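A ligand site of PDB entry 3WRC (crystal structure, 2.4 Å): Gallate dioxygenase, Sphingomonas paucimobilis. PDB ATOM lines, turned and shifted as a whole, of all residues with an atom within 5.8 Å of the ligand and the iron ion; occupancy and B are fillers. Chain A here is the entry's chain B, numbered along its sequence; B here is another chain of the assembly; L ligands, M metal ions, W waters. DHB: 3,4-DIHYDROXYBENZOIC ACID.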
ATOM      1  N   HIS A  12     -28.936   7.331 -25.971  1.00  0.00           N
ATOM      2  CA  HIS A  12     -28.640   7.451 -27.396  1.00  0.00           C
ATOM      3  C   HIS A  12     -27.400   8.316 -27.678  1.00  0.00           C
ATOM      4  O   HIS A  12     -27.111   8.667 -28.833  1.00  0.00           O
ATOM      5  CB  HIS A  12     -29.864   7.869 -28.220  1.00  0.00           C
ATOM      6  CG  HIS A  12     -30.363   9.266 -27.992  1.00  0.00           C
ATOM      7  ND1 HIS A  12     -31.706   9.577 -28.051  1.00  0.00           N
ATOM      8  CD2 HIS A  12     -29.716  10.436 -27.772  1.00  0.00           C
ATOM      9  CE1 HIS A  12     -31.873  10.870 -27.850  1.00  0.00           C
ATOM     10  NE2 HIS A  12     -30.677  11.420 -27.679  1.00  0.00           N
ATOM     11  N   THR A  13     -26.619   8.610 -26.647  1.00  0.00           N
ATOM     12  CA  THR A  13     -25.309   9.197 -26.850  1.00  0.00           C
ATOM     13  C   THR A  13     -24.510   8.622 -27.987  1.00  0.00           C
ATOM     14  O   THR A  13     -24.383   7.418 -28.124  1.00  0.00           O
ATOM     15  CB  THR A  13     -24.480   9.065 -25.587  1.00  0.00           C
ATOM     16  OG1 THR A  13     -24.972  10.058 -24.681  1.00  0.00           O
ATOM     17  CG2 THR A  13     -23.040   9.313 -25.860  1.00  0.00           C
ATOM     18  N   PRO A  14     -23.902   9.497 -28.790  1.00  0.00           N
ATOM     19  CA  PRO A  14     -23.118   9.056 -29.949  1.00  0.00           C
ATOM     20  C   PRO A  14     -21.994   8.126 -29.523  1.00  0.00           C
ATOM     21  O   PRO A  14     -21.485   7.380 -30.341  1.00  0.00           O
ATOM     22  CB  PRO A  14     -22.570  10.364 -30.559  1.00  0.00           C
ATOM     23  CG  PRO A  14     -22.666  11.373 -29.493  1.00  0.00           C
ATOM     24  CD  PRO A  14     -23.904  10.958 -28.658  1.00  0.00           C
ATOM     25  N   THR A  15     -21.599   8.147 -28.255  1.00  0.00           N
ATOM     26  CA  THR A  15     -20.502   7.245 -27.844  1.00  0.00           C
ATOM     27  C   THR A  15     -20.836   5.737 -27.992  1.00  0.00           C
ATOM     28  O   THR A  15     -19.947   4.919 -28.163  1.00  0.00           O
ATOM     29  CB  THR A  15     -19.987   7.542 -26.411  1.00  0.00           C
ATOM     30  OG1 THR A  15     -21.012   7.300 -25.431  1.00  0.00           O
ATOM     31  CG2 THR A  15     -19.517   8.983 -26.301  1.00  0.00           C
ATOM     32  N   ASN A  57     -34.820  12.240 -30.288  1.00  0.00           N
ATOM     33  CA  ASN A  57     -34.683  13.612 -30.733  1.00  0.00           C
ATOM     34  C   ASN A  57     -33.490  13.695 -31.627  1.00  0.00           C
ATOM     35  O   ASN A  57     -32.505  12.987 -31.405  1.00  0.00           O
ATOM     36  CB  ASN A  57     -34.482  14.578 -29.564  1.00  0.00           C
ATOM     37  CG  ASN A  57     -33.078  14.547 -29.042  1.00  0.00           C
ATOM     38  OD1 ASN A  57     -32.710  13.661 -28.257  1.00  0.00           O
ATOM     39  ND2 ASN A  57     -32.256  15.503 -29.494  1.00  0.00           N
ATOM     40  N   HIS A  59     -30.269  15.873 -33.205  1.00  0.00           N
ATOM     41  CA  HIS A  59     -29.363  16.885 -32.579  1.00  0.00           C
ATOM     42  C   HIS A  59     -28.845  18.003 -33.492  1.00  0.00           C
ATOM     43  O   HIS A  59     -27.658  18.093 -33.800  1.00  0.00           O
ATOM     44  CB  HIS A  59     -28.227  16.173 -31.841  1.00  0.00           C
ATOM     45  CG  HIS A  59     -28.734  15.197 -30.839  1.00  0.00           C
ATOM     46  ND1 HIS A  59     -29.285  13.986 -31.223  1.00  0.00           N
ATOM     47  CD2 HIS A  59     -28.892  15.285 -29.495  1.00  0.00           C
ATOM     48  CE1 HIS A  59     -29.726  13.350 -30.141  1.00  0.00           C
ATOM     49  NE2 HIS A  59     -29.493  14.109 -29.085  1.00  0.00           N
ATOM     50  N   HIS A 124     -27.415  10.309 -34.666  1.00  0.00           N
ATOM     51  CA  HIS A 124     -27.129   9.388 -33.576  1.00  0.00           C
ATOM     52  C   HIS A 124     -28.328   9.124 -32.653  1.00  0.00           C
ATOM     53  O   HIS A 124     -28.377   8.090 -32.008  1.00  0.00           O
ATOM     54  CB  HIS A 124     -25.880   9.795 -32.790  1.00  0.00           C
ATOM     55  CG  HIS A 124     -26.050  10.982 -31.885  1.00  0.00           C
ATOM     56  ND1 HIS A 124     -25.546  12.233 -32.189  1.00  0.00           N
ATOM     57  CD2 HIS A 124     -26.602  11.092 -30.656  1.00  0.00           C
ATOM     58  CE1 HIS A 124     -25.800  13.067 -31.190  1.00  0.00           C
ATOM     59  NE2 HIS A 124     -26.442  12.392 -30.250  1.00  0.00           N
ATOM     60  N   GLY A 125     -29.304  10.014 -32.592  1.00  0.00           N
ATOM     61  CA  GLY A 125     -30.452   9.786 -31.708  1.00  0.00           C
ATOM     62  C   GLY A 125     -31.169   8.471 -32.013  1.00  0.00           C
ATOM     63  O   GLY A 125     -31.793   7.854 -31.134  1.00  0.00           O
ATOM     64  N   VAL A 151     -36.933  18.421 -28.281  1.00  0.00           N
ATOM     65  CA  VAL A 151     -36.741  18.690 -26.874  1.00  0.00           C
ATOM     66  C   VAL A 151     -35.643  19.734 -26.648  1.00  0.00           C
ATOM     67  O   VAL A 151     -35.308  20.026 -25.508  1.00  0.00           O
ATOM     68  CB  VAL A 151     -36.294  17.404 -26.113  1.00  0.00           C
ATOM     69  CG1 VAL A 151     -37.428  16.370 -26.032  1.00  0.00           C
ATOM     70  CG2 VAL A 151     -34.997  16.816 -26.727  1.00  0.00           C
ATOM     71  N   LEU A 152     -35.046  20.253 -27.727  1.00  0.00           N
ATOM     72  CA  LEU A 152     -33.867  21.145 -27.579  1.00  0.00           C
ATOM     73  C   LEU A 152     -34.195  22.631 -27.542  1.00  0.00           C
ATOM     74  O   LEU A 152     -33.467  23.422 -26.959  1.00  0.00           O
ATOM     75  CB  LEU A 152     -32.856  20.902 -28.713  1.00  0.00           C
ATOM     76  CG  LEU A 152     -32.434  19.448 -28.863  1.00  0.00           C
ATOM     77  CD1 LEU A 152     -31.424  19.269 -29.989  1.00  0.00           C
ATOM     78  CD2 LEU A 152     -31.867  18.922 -27.531  1.00  0.00           C
ATOM     79  N   GLY A 188     -32.687   8.477 -25.243  1.00  0.00           N
ATOM     80  CA  GLY A 188     -32.107   9.692 -24.690  1.00  0.00           C
ATOM     81  C   GLY A 188     -31.761   9.518 -23.198  1.00  0.00           C
ATOM     82  O   GLY A 188     -32.161   8.513 -22.572  1.00  0.00           O
ATOM     83  N   GLY A 189     -31.048  10.487 -22.611  1.00  0.00           N
ATOM     84  CA  GLY A 189     -30.781  10.415 -21.184  1.00  0.00           C
ATOM     85  C   GLY A 189     -29.704   9.370 -20.883  1.00  0.00           C
ATOM     86  O   GLY A 189     -29.058   8.869 -21.825  1.00  0.00           O
ATOM     87  N   HIS A 192     -26.920  14.011 -17.958  1.00  0.00           N
ATOM     88  CA  HIS A 192     -25.742  14.555 -18.579  1.00  0.00           C
ATOM     89  C   HIS A 192     -25.992  15.993 -18.866  1.00  0.00           C
ATOM     90  O   HIS A 192     -27.139  16.416 -18.957  1.00  0.00           O
ATOM     91  CB  HIS A 192     -25.354  13.821 -19.869  1.00  0.00           C
ATOM     92  CG  HIS A 192     -26.374  13.880 -20.968  1.00  0.00           C
ATOM     93  ND1 HIS A 192     -27.628  13.317 -20.859  1.00  0.00           N
ATOM     94  CD2 HIS A 192     -26.275  14.341 -22.244  1.00  0.00           C
ATOM     95  CE1 HIS A 192     -28.283  13.465 -21.998  1.00  0.00           C
ATOM     96  NE2 HIS A 192     -27.481  14.072 -22.858  1.00  0.00           N
ATOM     97  N   VAL A 194     -23.954  18.605 -21.673  1.00  0.00           N
ATOM     98  CA  VAL A 194     -22.818  18.646 -22.578  1.00  0.00           C
ATOM     99  C   VAL A 194     -22.466  20.053 -23.024  1.00  0.00           C
ATOM    100  O   VAL A 194     -21.749  20.232 -24.013  1.00  0.00           O
ATOM    101  CB  VAL A 194     -23.042  17.736 -23.805  1.00  0.00           C
ATOM    102  CG1 VAL A 194     -22.766  16.291 -23.427  1.00  0.00           C
ATOM    103  CG2 VAL A 194     -24.458  17.864 -24.304  1.00  0.00           C
ATOM    104  N   GLU A 239     -34.029  15.601 -21.621  1.00  0.00           N
ATOM    105  CA  GLU A 239     -34.679  14.914 -22.739  1.00  0.00           C
ATOM    106  C   GLU A 239     -35.421  13.660 -22.262  1.00  0.00           C
ATOM    107  O   GLU A 239     -36.146  13.005 -23.032  1.00  0.00           O
ATOM    108  CB  GLU A 239     -33.686  14.596 -23.874  1.00  0.00           C
ATOM    109  CG  GLU A 239     -32.622  13.549 -23.502  1.00  0.00           C
ATOM    110  CD  GLU A 239     -31.562  13.324 -24.599  1.00  0.00           C
ATOM    111  OE1 GLU A 239     -31.807  13.594 -25.767  1.00  0.00           O
ATOM    112  OE2 GLU A 239     -30.465  12.849 -24.262  1.00  0.00           O
ATOM    113  N   MET A 242     -38.844  11.893 -23.111  1.00  0.00           N
ATOM    114  CA  MET A 242     -39.177  10.965 -24.177  1.00  0.00           C
ATOM    115  C   MET A 242     -39.399   9.534 -23.648  1.00  0.00           C
ATOM    116  O   MET A 242     -40.137   8.731 -24.244  1.00  0.00           O
ATOM    117  CB  MET A 242     -38.093  10.996 -25.259  1.00  0.00           C
ATOM    118  CG  MET A 242     -38.018  12.345 -25.952  1.00  0.00           C
ATOM    119  SD  MET A 242     -36.930  12.260 -27.380  1.00  0.00           S
ATOM    120  CE  MET A 242     -35.335  12.420 -26.546  1.00  0.00           C
ATOM    121  N   SER A 265     -18.263   8.258 -19.033  1.00  0.00           N
ATOM    122  CA  SER A 265     -17.798   9.636 -19.048  1.00  0.00           C
ATOM    123  C   SER A 265     -18.865  10.708 -18.868  1.00  0.00           C
ATOM    124  O   SER A 265     -19.123  11.147 -17.758  1.00  0.00           O
ATOM    125  CB  SER A 265     -16.894   9.944 -20.257  1.00  0.00           C
ATOM    126  OG  SER A 265     -17.447   9.463 -21.452  1.00  0.00           O
ATOM    127  N   MET A 266     -19.487  11.152 -19.957  1.00  0.00           N
ATOM    128  CA  MET A 266     -20.464  12.262 -19.862  1.00  0.00           C
ATOM    129  C   MET A 266     -21.899  11.844 -19.547  1.00  0.00           C
ATOM    130  O   MET A 266     -22.663  12.557 -18.849  1.00  0.00           O
ATOM    131  CB  MET A 266     -20.462  13.059 -21.166  1.00  0.00           C
ATOM    132  CG  MET A 266     -19.092  13.672 -21.558  1.00  0.00           C
ATOM    133  SD  MET A 266     -18.441  14.897 -20.333  1.00  0.00           S
ATOM    134  CE  MET A 266     -19.555  16.304 -20.625  1.00  0.00           C
ATOM    135  N   THR A 267     -22.271  10.687 -20.084  1.00  0.00           N
ATOM    136  CA  THR A 267     -23.639  10.298 -20.145  1.00  0.00           C
ATOM    137  C   THR A 267     -23.905   9.066 -19.321  1.00  0.00           C
ATOM    138  O   THR A 267     -23.127   8.090 -19.383  1.00  0.00           O
ATOM    139  CB  THR A 267     -24.021   9.917 -21.584  1.00  0.00           C
ATOM    140  OG1 THR A 267     -23.692  11.001 -22.472  1.00  0.00           O
ATOM    141  CG2 THR A 267     -25.542   9.578 -21.670  1.00  0.00           C
ATOM    142  N   PHE B 373     -24.745  23.405 -28.572  1.00  0.00           N
ATOM    143  CA  PHE B 373     -23.576  22.568 -28.465  1.00  0.00           C
ATOM    144  C   PHE B 373     -23.393  21.674 -29.690  1.00  0.00           C
ATOM    145  O   PHE B 373     -22.287  21.517 -30.202  1.00  0.00           O
ATOM    146  CB  PHE B 373     -23.639  21.721 -27.192  1.00  0.00           C
ATOM    147  CG  PHE B 373     -22.732  20.540 -27.236  1.00  0.00           C
ATOM    148  CD1 PHE B 373     -21.389  20.693 -27.070  1.00  0.00           C
ATOM    149  CD2 PHE B 373     -23.230  19.284 -27.503  1.00  0.00           C
ATOM    150  CE1 PHE B 373     -20.548  19.622 -27.135  1.00  0.00           C
ATOM    151  CE2 PHE B 373     -22.394  18.195 -27.580  1.00  0.00           C
ATOM    152  CZ  PHE B 373     -21.059  18.362 -27.388  1.00  0.00           C
ATOM    153  N   PHE B 374     -24.484  21.052 -30.111  1.00  0.00           N
ATOM    154  CA  PHE B 374     -24.485  20.159 -31.240  1.00  0.00           C
ATOM    155  C   PHE B 374     -23.913  20.740 -32.530  1.00  0.00           C
ATOM    156  O   PHE B 374     -23.366  19.988 -33.328  1.00  0.00           O
ATOM    157  CB  PHE B 374     -25.890  19.614 -31.417  1.00  0.00           C
ATOM    158  CG  PHE B 374     -26.507  19.125 -30.136  1.00  0.00           C
ATOM    159  CD1 PHE B 374     -26.086  17.945 -29.559  1.00  0.00           C
ATOM    160  CD2 PHE B 374     -27.490  19.856 -29.506  1.00  0.00           C
ATOM    161  CE1 PHE B 374     -26.653  17.491 -28.360  1.00  0.00           C
ATOM    162  CE2 PHE B 374     -28.059  19.405 -28.293  1.00  0.00           C
ATOM    163  CZ  PHE B 374     -27.642  18.230 -27.733  1.00  0.00           C
ATOM    164  N   GLU B 377     -20.217  20.367 -31.704  1.00  0.00           N
ATOM    165  CA  GLU B 377     -19.940  18.957 -31.972  1.00  0.00           C
ATOM    166  C   GLU B 377     -19.607  18.726 -33.459  1.00  0.00           C
ATOM    167  O   GLU B 377     -18.695  18.005 -33.785  1.00  0.00           O
ATOM    168  CB  GLU B 377     -21.182  18.125 -31.610  1.00  0.00           C
ATOM    169  CG  GLU B 377     -21.004  16.640 -31.771  1.00  0.00           C
ATOM    170  CD  GLU B 377     -22.110  15.866 -31.081  1.00  0.00           C
ATOM    171  OE1 GLU B 377     -23.307  16.124 -31.375  1.00  0.00           O
ATOM    172  OE2 GLU B 377     -21.805  15.004 -30.234  1.00  0.00           O
ATOM    173  N   ASN B 387     -15.146  15.735 -28.794  1.00  0.00           N
ATOM    174  CA  ASN B 387     -16.064  16.326 -27.846  1.00  0.00           C
ATOM    175  C   ASN B 387     -15.387  16.576 -26.533  1.00  0.00           C
ATOM    176  O   ASN B 387     -15.724  17.540 -25.844  1.00  0.00           O
ATOM    177  CB  ASN B 387     -17.269  15.420 -27.574  1.00  0.00           C
ATOM    178  CG  ASN B 387     -18.209  15.330 -28.736  1.00  0.00           C
ATOM    179  OD1 ASN B 387     -17.797  15.447 -29.873  1.00  0.00           O
ATOM    180  ND2 ASN B 387     -19.482  15.099 -28.458  1.00  0.00           N
ATOM    181  N   TYR B 391     -15.450  19.680 -24.099  1.00  0.00           N
ATOM    182  CA  TYR B 391     -15.967  19.682 -22.721  1.00  0.00           C
ATOM    183  C   TYR B 391     -14.893  20.246 -21.789  1.00  0.00           C
ATOM    184  O   TYR B 391     -15.156  21.133 -20.976  1.00  0.00           O
ATOM    185  CB  TYR B 391     -16.370  18.290 -22.276  1.00  0.00           C
ATOM    186  CG  TYR B 391     -17.395  17.616 -23.188  1.00  0.00           C
ATOM    187  CD1 TYR B 391     -18.439  18.342 -23.739  1.00  0.00           C
ATOM    188  CD2 TYR B 391     -17.306  16.283 -23.476  1.00  0.00           C
ATOM    189  CE1 TYR B 391     -19.387  17.738 -24.541  1.00  0.00           C
ATOM    190  CE2 TYR B 391     -18.237  15.665 -24.281  1.00  0.00           C
ATOM    191  CZ  TYR B 391     -19.290  16.394 -24.797  1.00  0.00           C
ATOM    192  OH  TYR B 391     -20.218  15.784 -25.625  1.00  0.00           O
ATOM    193  N   TYR B 412     -13.354  10.337 -28.732  1.00  0.00           N
ATOM    194  CA  TYR B 412     -14.371  10.103 -29.777  1.00  0.00           C
ATOM    195  C   TYR B 412     -14.914  11.412 -30.393  1.00  0.00           C
ATOM    196  O   TYR B 412     -14.867  12.462 -29.757  1.00  0.00           O
ATOM    197  CB  TYR B 412     -15.534   9.321 -29.157  1.00  0.00           C
ATOM    198  CG  TYR B 412     -16.263  10.081 -28.058  1.00  0.00           C
ATOM    199  CD1 TYR B 412     -17.373  10.884 -28.348  1.00  0.00           C
ATOM    200  CD2 TYR B 412     -15.834  10.017 -26.733  1.00  0.00           C
ATOM    201  CE1 TYR B 412     -18.029  11.608 -27.337  1.00  0.00           C
ATOM    202  CE2 TYR B 412     -16.485  10.719 -25.724  1.00  0.00           C
ATOM    203  CZ  TYR B 412     -17.588  11.511 -26.026  1.00  0.00           C
ATOM    204  OH  TYR B 412     -18.239  12.189 -25.012  1.00  0.00           O
HETATM  205  C1  DHB L   1     -22.903  13.148 -25.778  1.00  0.00           C
HETATM  206  C2  DHB L   1     -22.852  13.879 -26.947  1.00  0.00           C
HETATM  207  C3  DHB L   1     -24.040  14.164 -27.617  1.00  0.00           C
HETATM  208  O3  DHB L   1     -24.014  14.882 -28.772  1.00  0.00           O
HETATM  209  C4  DHB L   1     -25.247  13.721 -27.100  1.00  0.00           C
HETATM  210  O4  DHB L   1     -26.425  13.953 -27.764  1.00  0.00           O
HETATM  211  C5  DHB L   1     -25.286  12.971 -25.940  1.00  0.00           C
HETATM  212  C6  DHB L   1     -24.108  12.688 -25.279  1.00  0.00           C
HETATM  213  C   DHB L   1     -21.620  12.814 -25.024  1.00  0.00           C
HETATM  214  O1  DHB L   1     -20.579  13.413 -25.372  1.00  0.00           O
HETATM  215  O2  DHB L   1     -21.653  11.789 -24.292  1.00  0.00           O
HETATM  216 FE    FE M   1     -30.718  13.468 -27.433  1.00  0.00          FE
HETATM  217  O   HOH W   1     -30.431  15.425 -26.933  1.00  0.00           O
HETATM  218  O   HOH W   2     -29.058  13.254 -26.362  1.00  0.00           O
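NE2 of His 59 sits close to O4 of the ligand (3.3 Å).
O1 of the ligand is in hydrogen-bond range of OH of Tyr 391 of chain B.
OE2 of Glu 377 of chain B lies within hydrogen-bond range of O3 of the ligand (2.7 Å).
An oxygen (O1) of the ligand lies within hydrogen-bond range of the side-chain hydroxyl (OH) of Tyr 412 of chain B (2.7 Å).
O2 of the ligand sits at hydrogen-bond distance from OG1 of Thr 267 (2.8 Å).
NE2 of His 124 lies within hydrogen-bond range of O4 of the ligand, 2.9 Å away.
The backbone NH (N) of Gly 189 lies within hydrogen-bond range of the side-chain carboxylate (OE2) of Glu 239 (2.9 Å).
A ring nitrogen (ND1) of His 12 lies within hydrogen-bond range of the backbone NH (N) of Gly 188, at 3.2 Å.
A ring nitrogen (ND1) of His 59 sits at hydrogen-bond distance from a ring nitrogen (NE2) of His 124 (3.4 Å).
N of Asn 57 lies within hydrogen-bond range of SD of Met 242, 3.6 Å away.
The side-chain hydroxyl of Tyr 391 of chain B sits at hydrogen-bond distance from the side-chain amide nitrogen of Asn 387 of chain B (3.0 Å).
OE2 of Glu 377 of chain B is in hydrogen-bond range of ND2 of Asn 387 of chain B, 2.9 Å away.
The backbone carbonyl oxygen of Tyr 412 of chain B lies within hydrogen-bond range of the backbone NH of Asn 387 of chain B, 3.4 Å away.
OG1 of Thr 13 lies within hydrogen-bond range of OG1 of Thr 267 (2.7 Å).
Thr 13 touches the ligand.
Pro 14 touches the ligand.
His 192 touches the ligand (NE2 to C5, 3.9 Å).
Val 194 touches the ligand (CG1 to C1, 3.9 Å).
Met 266 touches the ligand (CB to O2, 3.6 Å).
Phe 373 of chain B touches the ligand (CE2 to O3, 3.9 Å).
CE1 of Phe 374 of chain B touches O4 of the ligand, at 3.6 Å.
Asn 387 of chain B touches the ligand (ND2 to O1, 3.7 Å).
Hydrophobic or aromatic side chains that line the ligand: Pro 14, His 59, His 124, Val 194, Met 266, Phe 373 of chain B, Phe 374 of chain B, Tyr 391 of chain B and Tyr 412 of chain B.
14 residues have an atom within 4 Å of the ligand: Thr 13, Pro 14, His 59, His 124, His 192, Val 194, Met 266, Thr 267, Phe 373 of chain B, Phe 374 of chain B, Glu 377 of chain B, Asn 387 of chain B, Tyr 391 of chain B and Tyr 412 of chain B.
Four residues have an atom within 4 Å of the iron ion: His 12, Asn 57, His 59 and Glu 239.
The nearest printed residue that does not touch the iron ion is Met 242 (4.8 Å).
Water W2 binds the iron ion.
OE1 of Glu 239 is bound to the iron ion, 2.0 Å away.
The iron ion is bound by water W1 (2.0 Å).
The iron ion is bound by NE2 of His 12, 2.1 Å away.
The iron ion is bound by a ring nitrogen (NE2) of His 59 (2.2 Å).
The iron ion is bound by OD1 of Asn 57, 2.2 Å away.
Water W2 lies within hydrogen-bond range of the side-chain carboxylate (OE2) of Glu 239 (2.6 Å) and an oxygen (O4) of the ligand (3.1 Å).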
